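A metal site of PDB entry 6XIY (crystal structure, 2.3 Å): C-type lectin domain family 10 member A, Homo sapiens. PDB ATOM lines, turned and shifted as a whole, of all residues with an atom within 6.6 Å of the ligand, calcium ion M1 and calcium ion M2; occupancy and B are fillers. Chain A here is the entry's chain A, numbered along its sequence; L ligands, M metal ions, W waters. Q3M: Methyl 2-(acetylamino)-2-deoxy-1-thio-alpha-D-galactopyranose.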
ATOM      1  N   TYR A  57     -16.575  29.038   5.599  1.00  0.00           N
ATOM      2  CA  TYR A  57     -15.932  27.699   5.695  1.00  0.00           C
ATOM      3  C   TYR A  57     -14.543  27.797   5.080  1.00  0.00           C
ATOM      4  O   TYR A  57     -14.438  28.384   3.989  1.00  0.00           O
ATOM      5  CB  TYR A  57     -16.786  26.617   5.023  1.00  0.00           C
ATOM      6  CG  TYR A  57     -18.151  26.436   5.641  1.00  0.00           C
ATOM      7  CD1 TYR A  57     -18.372  26.650   6.996  1.00  0.00           C
ATOM      8  CD2 TYR A  57     -19.235  26.074   4.862  1.00  0.00           C
ATOM      9  CE1 TYR A  57     -19.624  26.506   7.549  1.00  0.00           C
ATOM     10  CE2 TYR A  57     -20.494  25.881   5.402  1.00  0.00           C
ATOM     11  CZ  TYR A  57     -20.692  26.098   6.756  1.00  0.00           C
ATOM     12  OH  TYR A  57     -21.918  25.884   7.272  1.00  0.00           O
ATOM     13  N   ASP A  64      -8.513  12.469   5.075  1.00  0.00           N
ATOM     14  CA  ASP A  64      -8.557  10.999   5.338  1.00  0.00           C
ATOM     15  C   ASP A  64      -8.947  10.251   4.065  1.00  0.00           C
ATOM     16  O   ASP A  64      -9.728   9.310   4.151  1.00  0.00           O
ATOM     17  CB  ASP A  64      -9.528  10.657   6.482  1.00  0.00           C
ATOM     18  CG  ASP A  64     -11.015  10.731   6.171  1.00  0.00           C
ATOM     19  OD1 ASP A  64     -11.417  11.444   5.222  1.00  0.00           O
ATOM     20  OD2 ASP A  64     -11.824  10.078   6.861  1.00  0.00           O
ATOM     21  N   PRO A  65      -8.417  10.590   2.869  1.00  0.00           N
ATOM     22  CA  PRO A  65      -8.842   9.916   1.635  1.00  0.00           C
ATOM     23  C   PRO A  65      -8.492   8.415   1.679  1.00  0.00           C
ATOM     24  O   PRO A  65      -9.286   7.611   1.212  1.00  0.00           O
ATOM     25  CB  PRO A  65      -8.095  10.653   0.502  1.00  0.00           C
ATOM     26  CG  PRO A  65      -6.914  11.292   1.204  1.00  0.00           C
ATOM     27  CD  PRO A  65      -7.400  11.617   2.604  1.00  0.00           C
ATOM     28  N   GLY A  67      -8.443   6.491   4.405  1.00  0.00           N
ATOM     29  CA  GLY A  67      -9.099   5.796   5.544  1.00  0.00           C
ATOM     30  C   GLY A  67      -8.793   6.399   6.912  1.00  0.00           C
ATOM     31  O   GLY A  67      -9.731   6.421   7.738  1.00  0.00           O
ATOM     32  N   TRP A  69      -7.206   9.774   9.294  1.00  0.00           N
ATOM     33  CA  TRP A  69      -6.957  11.245   9.299  1.00  0.00           C
ATOM     34  C   TRP A  69      -5.459  11.550   9.344  1.00  0.00           C
ATOM     35  O   TRP A  69      -4.786  10.950  10.163  1.00  0.00           O
ATOM     36  CB  TRP A  69      -7.692  11.933  10.439  1.00  0.00           C
ATOM     37  CG  TRP A  69      -9.154  12.007  10.167  1.00  0.00           C
ATOM     38  CD1 TRP A  69     -10.128  11.178  10.635  1.00  0.00           C
ATOM     39  CD2 TRP A  69      -9.795  12.938   9.278  1.00  0.00           C
ATOM     40  NE1 TRP A  69     -11.337  11.557  10.126  1.00  0.00           N
ATOM     41  CE2 TRP A  69     -11.166  12.618   9.275  1.00  0.00           C
ATOM     42  CE3 TRP A  69      -9.339  13.983   8.468  1.00  0.00           C
ATOM     43  CZ2 TRP A  69     -12.086  13.322   8.509  1.00  0.00           C
ATOM     44  CZ3 TRP A  69     -10.260  14.676   7.721  1.00  0.00           C
ATOM     45  CH2 TRP A  69     -11.612  14.349   7.736  1.00  0.00           C
ATOM     46  N   LYS A  85     -16.673  19.708  15.526  1.00  0.00           N
ATOM     47  CA  LYS A  85     -18.106  19.981  15.778  1.00  0.00           C
ATOM     48  C   LYS A  85     -18.736  18.749  16.426  1.00  0.00           C
ATOM     49  O   LYS A  85     -18.315  17.644  16.102  1.00  0.00           O
ATOM     50  CB  LYS A  85     -18.843  20.245  14.458  1.00  0.00           C
ATOM     51  CG  LYS A  85     -18.910  21.688  13.999  1.00  0.00           C
ATOM     52  CD  LYS A  85     -19.846  22.557  14.803  1.00  0.00           C
ATOM     53  CE  LYS A  85     -20.195  23.836  14.061  1.00  0.00           C
ATOM     54  NZ  LYS A  85     -20.353  25.003  14.955  1.00  0.00           N
ATOM     55  N   GLY A  87     -20.832  15.604  16.525  1.00  0.00           N
ATOM     56  CA  GLY A  87     -21.277  14.663  15.484  1.00  0.00           C
ATOM     57  C   GLY A  87     -20.242  14.473  14.379  1.00  0.00           C
ATOM     58  O   GLY A  87     -20.429  13.580  13.556  1.00  0.00           O
ATOM     59  N   GLN A  88     -19.166  15.266  14.355  1.00  0.00           N
ATOM     60  CA  GLN A  88     -18.113  15.173  13.316  1.00  0.00           C
ATOM     61  C   GLN A  88     -16.874  14.515  13.913  1.00  0.00           C
ATOM     62  O   GLN A  88     -16.652  14.572  15.128  1.00  0.00           O
ATOM     63  CB  GLN A  88     -17.906  16.561  12.685  1.00  0.00           C
ATOM     64  CG  GLN A  88     -19.209  17.253  12.295  1.00  0.00           C
ATOM     65  CD  GLN A  88     -19.925  16.614  11.112  1.00  0.00           C
ATOM     66  OE1 GLN A  88     -19.375  15.768  10.405  1.00  0.00           O
ATOM     67  NE2 GLN A  88     -21.153  17.062  10.841  1.00  0.00           N
ATOM     68  N   PRO A  89     -16.033  13.838  13.099  1.00  0.00           N
ATOM     69  CA  PRO A  89     -16.292  13.666  11.667  1.00  0.00           C
ATOM     70  C   PRO A  89     -17.298  12.522  11.432  1.00  0.00           C
ATOM     71  O   PRO A  89     -17.402  11.712  12.307  1.00  0.00           O
ATOM     72  CB  PRO A  89     -14.904  13.338  11.123  1.00  0.00           C
ATOM     73  CG  PRO A  89     -14.169  12.649  12.263  1.00  0.00           C
ATOM     74  CD  PRO A  89     -14.795  13.188  13.536  1.00  0.00           C
ATOM     75  N   ASP A  90     -18.048  12.537  10.326  1.00  0.00           N
ATOM     76  CA  ASP A  90     -19.165  11.568  10.080  1.00  0.00           C
ATOM     77  C   ASP A  90     -19.034  10.878   8.708  1.00  0.00           C
ATOM     78  O   ASP A  90     -19.889  10.032   8.434  1.00  0.00           O
ATOM     79  CB  ASP A  90     -20.542  12.232  10.165  1.00  0.00           C
ATOM     80  CG  ASP A  90     -20.762  13.392   9.185  1.00  0.00           C
ATOM     81  OD1 ASP A  90     -19.789  13.820   8.459  1.00  0.00           O
ATOM     82  OD2 ASP A  90     -21.914  13.877   9.162  1.00  0.00           O
ATOM     83  N   ASP A  91     -18.088  11.289   7.862  1.00  0.00           N
ATOM     84  CA  ASP A  91     -17.910  10.773   6.479  1.00  0.00           C
ATOM     85  C   ASP A  91     -19.274  10.698   5.738  1.00  0.00           C
ATOM     86  O   ASP A  91     -19.520   9.693   5.031  1.00  0.00           O
ATOM     87  CB  ASP A  91     -17.203   9.413   6.540  1.00  0.00           C
ATOM     88  CG  ASP A  91     -16.567   8.980   5.213  1.00  0.00           C
ATOM     89  OD1 ASP A  91     -15.808   9.805   4.598  1.00  0.00           O
ATOM     90  OD2 ASP A  91     -16.796   7.817   4.836  1.00  0.00           O
ATOM     91  N   TRP A  92     -20.147  11.703   5.884  1.00  0.00           N
ATOM     92  CA  TRP A  92     -21.545  11.726   5.333  1.00  0.00           C
ATOM     93  C   TRP A  92     -21.547  11.426   3.836  1.00  0.00           C
ATOM     94  O   TRP A  92     -20.640  11.959   3.151  1.00  0.00           O
ATOM     95  CB  TRP A  92     -22.147  13.098   5.578  1.00  0.00           C
ATOM     96  CG  TRP A  92     -23.615  13.236   5.351  1.00  0.00           C
ATOM     97  CD1 TRP A  92     -24.595  12.420   5.819  1.00  0.00           C
ATOM     98  CD2 TRP A  92     -24.278  14.323   4.685  1.00  0.00           C
ATOM     99  NE1 TRP A  92     -25.820  12.903   5.450  1.00  0.00           N
ATOM    100  CE2 TRP A  92     -25.660  14.077   4.758  1.00  0.00           C
ATOM    101  CE3 TRP A  92     -23.847  15.476   4.014  1.00  0.00           C
ATOM    102  CZ2 TRP A  92     -26.615  14.933   4.195  1.00  0.00           C
ATOM    103  CZ3 TRP A  92     -24.789  16.336   3.472  1.00  0.00           C
ATOM    104  CH2 TRP A  92     -26.157  16.064   3.561  1.00  0.00           C
ATOM    105  N   GLY A 100     -17.788   9.768   0.585  1.00  0.00           N
ATOM    106  CA  GLY A 100     -18.143  10.381   1.876  1.00  0.00           C
ATOM    107  C   GLY A 100     -17.636  11.813   1.943  1.00  0.00           C
ATOM    108  O   GLY A 100     -17.968  12.627   1.036  1.00  0.00           O
ATOM    109  N   GLU A 101     -16.857  12.120   2.968  1.00  0.00           N
ATOM    110  CA  GLU A 101     -16.272  13.451   3.244  1.00  0.00           C
ATOM    111  C   GLU A 101     -14.840  13.228   3.748  1.00  0.00           C
ATOM    112  O   GLU A 101     -14.677  12.491   4.721  1.00  0.00           O
ATOM    113  CB  GLU A 101     -17.157  14.197   4.257  1.00  0.00           C
ATOM    114  CG  GLU A 101     -18.554  14.525   3.737  1.00  0.00           C
ATOM    115  CD  GLU A 101     -19.387  15.307   4.739  1.00  0.00           C
ATOM    116  OE1 GLU A 101     -19.205  15.028   5.953  1.00  0.00           O
ATOM    117  OE2 GLU A 101     -20.193  16.220   4.322  1.00  0.00           O
ATOM    118  N   ASP A 102     -13.844  13.774   3.059  1.00  0.00           N
ATOM    119  CA  ASP A 102     -12.431  13.392   3.252  1.00  0.00           C
ATOM    120  C   ASP A 102     -11.539  14.596   3.519  1.00  0.00           C
ATOM    121  O   ASP A 102     -10.340  14.388   3.608  1.00  0.00           O
ATOM    122  CB  ASP A 102     -11.923  12.617   2.031  1.00  0.00           C
ATOM    123  CG  ASP A 102     -12.635  11.280   1.914  1.00  0.00           C
ATOM    124  OD1 ASP A 102     -13.316  10.853   2.943  1.00  0.00           O
ATOM    125  OD2 ASP A 102     -12.546  10.675   0.822  1.00  0.00           O
ATOM    126  N   CYS A 103     -12.110  15.791   3.709  1.00  0.00           N
ATOM    127  CA  CYS A 103     -11.363  17.060   3.890  1.00  0.00           C
ATOM    128  C   CYS A 103     -12.019  17.859   5.022  1.00  0.00           C
ATOM    129  O   CYS A 103     -13.255  17.893   5.064  1.00  0.00           O
ATOM    130  CB  CYS A 103     -11.357  17.850   2.588  1.00  0.00           C
ATOM    131  SG  CYS A 103     -10.331  17.088   1.304  1.00  0.00           S
ATOM    132  N   HIS A 105     -12.554  21.341   7.447  1.00  0.00           N
ATOM    133  CA  HIS A 105     -12.590  22.809   7.361  1.00  0.00           C
ATOM    134  C   HIS A 105     -13.029  23.354   8.692  1.00  0.00           C
ATOM    135  O   HIS A 105     -13.715  22.646   9.421  1.00  0.00           O
ATOM    136  CB  HIS A 105     -13.526  23.250   6.226  1.00  0.00           C
ATOM    137  CG  HIS A 105     -14.960  22.962   6.470  1.00  0.00           C
ATOM    138  ND1 HIS A 105     -15.813  23.886   7.051  1.00  0.00           N
ATOM    139  CD2 HIS A 105     -15.716  21.881   6.182  1.00  0.00           C
ATOM    140  CE1 HIS A 105     -17.032  23.373   7.124  1.00  0.00           C
ATOM    141  NE2 HIS A 105     -17.000  22.148   6.585  1.00  0.00           N
ATOM    142  N   HIS A 107     -15.622  25.801  10.677  1.00  0.00           N
ATOM    143  CA  HIS A 107     -16.810  26.686  10.735  1.00  0.00           C
ATOM    144  C   HIS A 107     -16.332  28.043  11.250  1.00  0.00           C
ATOM    145  O   HIS A 107     -15.236  28.156  11.809  1.00  0.00           O
ATOM    146  CB  HIS A 107     -17.910  26.093  11.618  1.00  0.00           C
ATOM    147  CG  HIS A 107     -18.678  24.968  11.007  1.00  0.00           C
ATOM    148  ND1 HIS A 107     -20.034  25.023  10.808  1.00  0.00           N
ATOM    149  CD2 HIS A 107     -18.288  23.729  10.615  1.00  0.00           C
ATOM    150  CE1 HIS A 107     -20.468  23.884  10.305  1.00  0.00           C
ATOM    151  NE2 HIS A 107     -19.403  23.066  10.169  1.00  0.00           N
ATOM    152  N   ASN A 113     -15.367  20.436  10.690  1.00  0.00           N
ATOM    153  CA  ASN A 113     -16.292  19.485  10.021  1.00  0.00           C
ATOM    154  C   ASN A 113     -15.518  18.783   8.898  1.00  0.00           C
ATOM    155  O   ASN A 113     -14.602  19.402   8.349  1.00  0.00           O
ATOM    156  CB  ASN A 113     -17.550  20.188   9.508  1.00  0.00           C
ATOM    157  CG  ASN A 113     -18.370  19.297   8.596  1.00  0.00           C
ATOM    158  OD1 ASN A 113     -18.731  18.175   8.973  1.00  0.00           O
ATOM    159  ND2 ASN A 113     -18.617  19.757   7.378  1.00  0.00           N
ATOM    160  N   ASP A 114     -15.855  17.537   8.582  1.00  0.00           N
ATOM    161  CA  ASP A 114     -15.397  16.875   7.332  1.00  0.00           C
ATOM    162  C   ASP A 114     -16.443  17.109   6.230  1.00  0.00           C
ATOM    163  O   ASP A 114     -17.678  17.078   6.539  1.00  0.00           O
ATOM    164  CB  ASP A 114     -15.116  15.381   7.532  1.00  0.00           C
ATOM    165  CG  ASP A 114     -16.282  14.544   8.021  1.00  0.00           C
ATOM    166  OD1 ASP A 114     -17.256  15.139   8.617  1.00  0.00           O
ATOM    167  OD2 ASP A 114     -16.218  13.291   7.840  1.00  0.00           O
ATOM    168  N   ASP A 115     -15.947  17.438   5.046  1.00  0.00           N
ATOM    169  CA  ASP A 115     -16.761  17.870   3.883  1.00  0.00           C
ATOM    170  C   ASP A 115     -16.090  17.337   2.617  1.00  0.00           C
ATOM    171  O   ASP A 115     -14.964  16.731   2.703  1.00  0.00           O
ATOM    172  CB  ASP A 115     -16.956  19.391   3.830  1.00  0.00           C
ATOM    173  CG  ASP A 115     -18.335  19.860   3.329  1.00  0.00           C
ATOM    174  OD1 ASP A 115     -18.925  19.162   2.475  1.00  0.00           O
ATOM    175  OD2 ASP A 115     -18.810  20.924   3.805  1.00  0.00           O
ATOM    176  N   VAL A 116     -16.788  17.567   1.513  1.00  0.00           N
ATOM    177  CA  VAL A 116     -16.437  17.117   0.143  1.00  0.00           C
ATOM    178  C   VAL A 116     -15.310  18.021  -0.329  1.00  0.00           C
ATOM    179  O   VAL A 116     -15.503  19.252  -0.322  1.00  0.00           O
ATOM    180  CB  VAL A 116     -17.681  17.188  -0.766  1.00  0.00           C
ATOM    181  CG1 VAL A 116     -17.356  16.805  -2.210  1.00  0.00           C
ATOM    182  CG2 VAL A 116     -18.801  16.311  -0.212  1.00  0.00           C
ATOM    183  N   TYR A 121     -13.855  26.497  -0.951  1.00  0.00           N
ATOM    184  CA  TYR A 121     -13.849  27.131   0.389  1.00  0.00           C
ATOM    185  C   TYR A 121     -12.610  28.020   0.521  1.00  0.00           C
ATOM    186  O   TYR A 121     -11.638  27.868  -0.256  1.00  0.00           O
ATOM    187  CB  TYR A 121     -13.832  26.057   1.488  1.00  0.00           C
ATOM    188  CG  TYR A 121     -15.113  25.311   1.771  1.00  0.00           C
ATOM    189  CD1 TYR A 121     -16.340  25.747   1.318  1.00  0.00           C
ATOM    190  CD2 TYR A 121     -15.096  24.167   2.554  1.00  0.00           C
ATOM    191  CE1 TYR A 121     -17.511  25.068   1.617  1.00  0.00           C
ATOM    192  CE2 TYR A 121     -16.256  23.484   2.873  1.00  0.00           C
ATOM    193  CZ  TYR A 121     -17.477  23.939   2.411  1.00  0.00           C
ATOM    194  OH  TYR A 121     -18.632  23.276   2.711  1.00  0.00           O
HETATM  195  C01 Q3M L   1     -26.469  19.649   6.672  1.00  0.00           C
HETATM  196  S02 Q3M L   1     -24.677  19.681   6.308  1.00  0.00           S
HETATM  197  C03 Q3M L   1     -23.638  19.294   7.801  1.00  0.00           C
HETATM  198  C04 Q3M L   1     -24.108  18.065   8.560  1.00  0.00           C
HETATM  199  C05 Q3M L   1     -23.939  16.842   7.650  1.00  0.00           C
HETATM  200  C06 Q3M L   1     -24.555  15.602   8.358  1.00  0.00           C
HETATM  201  O07 Q3M L   1     -25.934  15.858   8.565  1.00  0.00           O
HETATM  202  C08 Q3M L   1     -22.483  16.591   7.208  1.00  0.00           C
HETATM  203  O09 Q3M L   1     -21.561  16.203   8.226  1.00  0.00           O
HETATM  204  C10 Q3M L   1     -21.831  17.825   6.578  1.00  0.00           C
HETATM  205  O11 Q3M L   1     -20.437  17.534   6.558  1.00  0.00           O
HETATM  206  C12 Q3M L   1     -22.138  19.068   7.417  1.00  0.00           C
HETATM  207  N13 Q3M L   1     -21.798  20.257   6.654  1.00  0.00           N
HETATM  208  C14 Q3M L   1     -21.210  21.399   7.328  1.00  0.00           C
HETATM  209  C15 Q3M L   1     -20.865  22.602   6.455  1.00  0.00           C
HETATM  210  O16 Q3M L   1     -20.951  21.360   8.494  1.00  0.00           O
HETATM  211 CA    CA M   1     -19.243  16.088   8.028  1.00  0.00          CA
HETATM  212 CA    CA M   2     -13.623  10.468   5.277  1.00  0.00          CA
HETATM  213  O   HOH W   1     -21.807  20.672   3.981  1.00  0.00           O
HETATM  214  O   HOH W   2     -14.639  11.236   7.254  1.00  0.00           O
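The side-chain carboxylate (OD1) of Asp 114 is bound to calcium ion M1, at 2.3 Å.
O09 of the ligand binds calcium ion M1 (2.3 Å).
The side-chain carboxylate (OE1) of Glu 101 is bound to calcium ion M1, 2.3 Å away.
Calcium ion M1 is bound by OD1 of Asn 113 (2.3 Å).
Calcium ion M1 is bound by OD1 of Asp 90 (2.4 Å).
O of Asp 114 is bound to calcium ion M1, 2.4 Å away.
Calcium ion M1 is bound by O11 of the ligand (2.4 Å).
Calcium ion M1 is bound by the side-chain amide oxygen (OE1) of Gln 88 (2.4 Å).
Calcium ion M1 has eight donor atoms within binding distance.
O of Asn 113 lies within hydrogen-bond range of N of His 105, 3.0 Å away.
O of Cys 103 sits at hydrogen-bond distance from N of Asp 115 (2.7 Å).
OH of Tyr 121 lies within hydrogen-bond range of OD2 of Asp 115.
The backbone NH (N) of Asp 102 sits at hydrogen-bond distance from the backbone carbonyl oxygen (O) of Asp 115 (3.2 Å).
The side-chain carboxylate (OD1) of Asp 90 lies close to the backbone NH (N) of Trp 92 (3.4 Å).
The backbone NH (N) of Asp 91 sits at hydrogen-bond distance from the side-chain carboxylate (OD2) of Asp 114 (2.7 Å).
The side-chain carboxylate (OE1) of Glu 101 sits close to the backbone NH (N) of Trp 92.
Of the 23 residues printed, 4 come within 4 Å of calcium ion M2.
The nearest printed residue that does not touch calcium ion M2 is Trp 69 (4.6 Å).
O16 of the ligand sits at hydrogen-bond distance from NE2 of His 107 (2.8 Å).
Merely in contact with the ligand: Tyr 57, Trp 92, Asp 115 and His 105.
Calcium ion M2 is bound by O of Glu 101, water W2, OD1 of Asp 91, OD1 of Asp 102, OD1 of Asp 64 and OD2 of Asp 64.
Calcium ion M2 has six donor atoms within binding distance.
Water W1 bridges a nitrogen (N13) of the ligand (2.7 Å) and the side-chain carboxylate of Asp 115 (3.0 Å).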
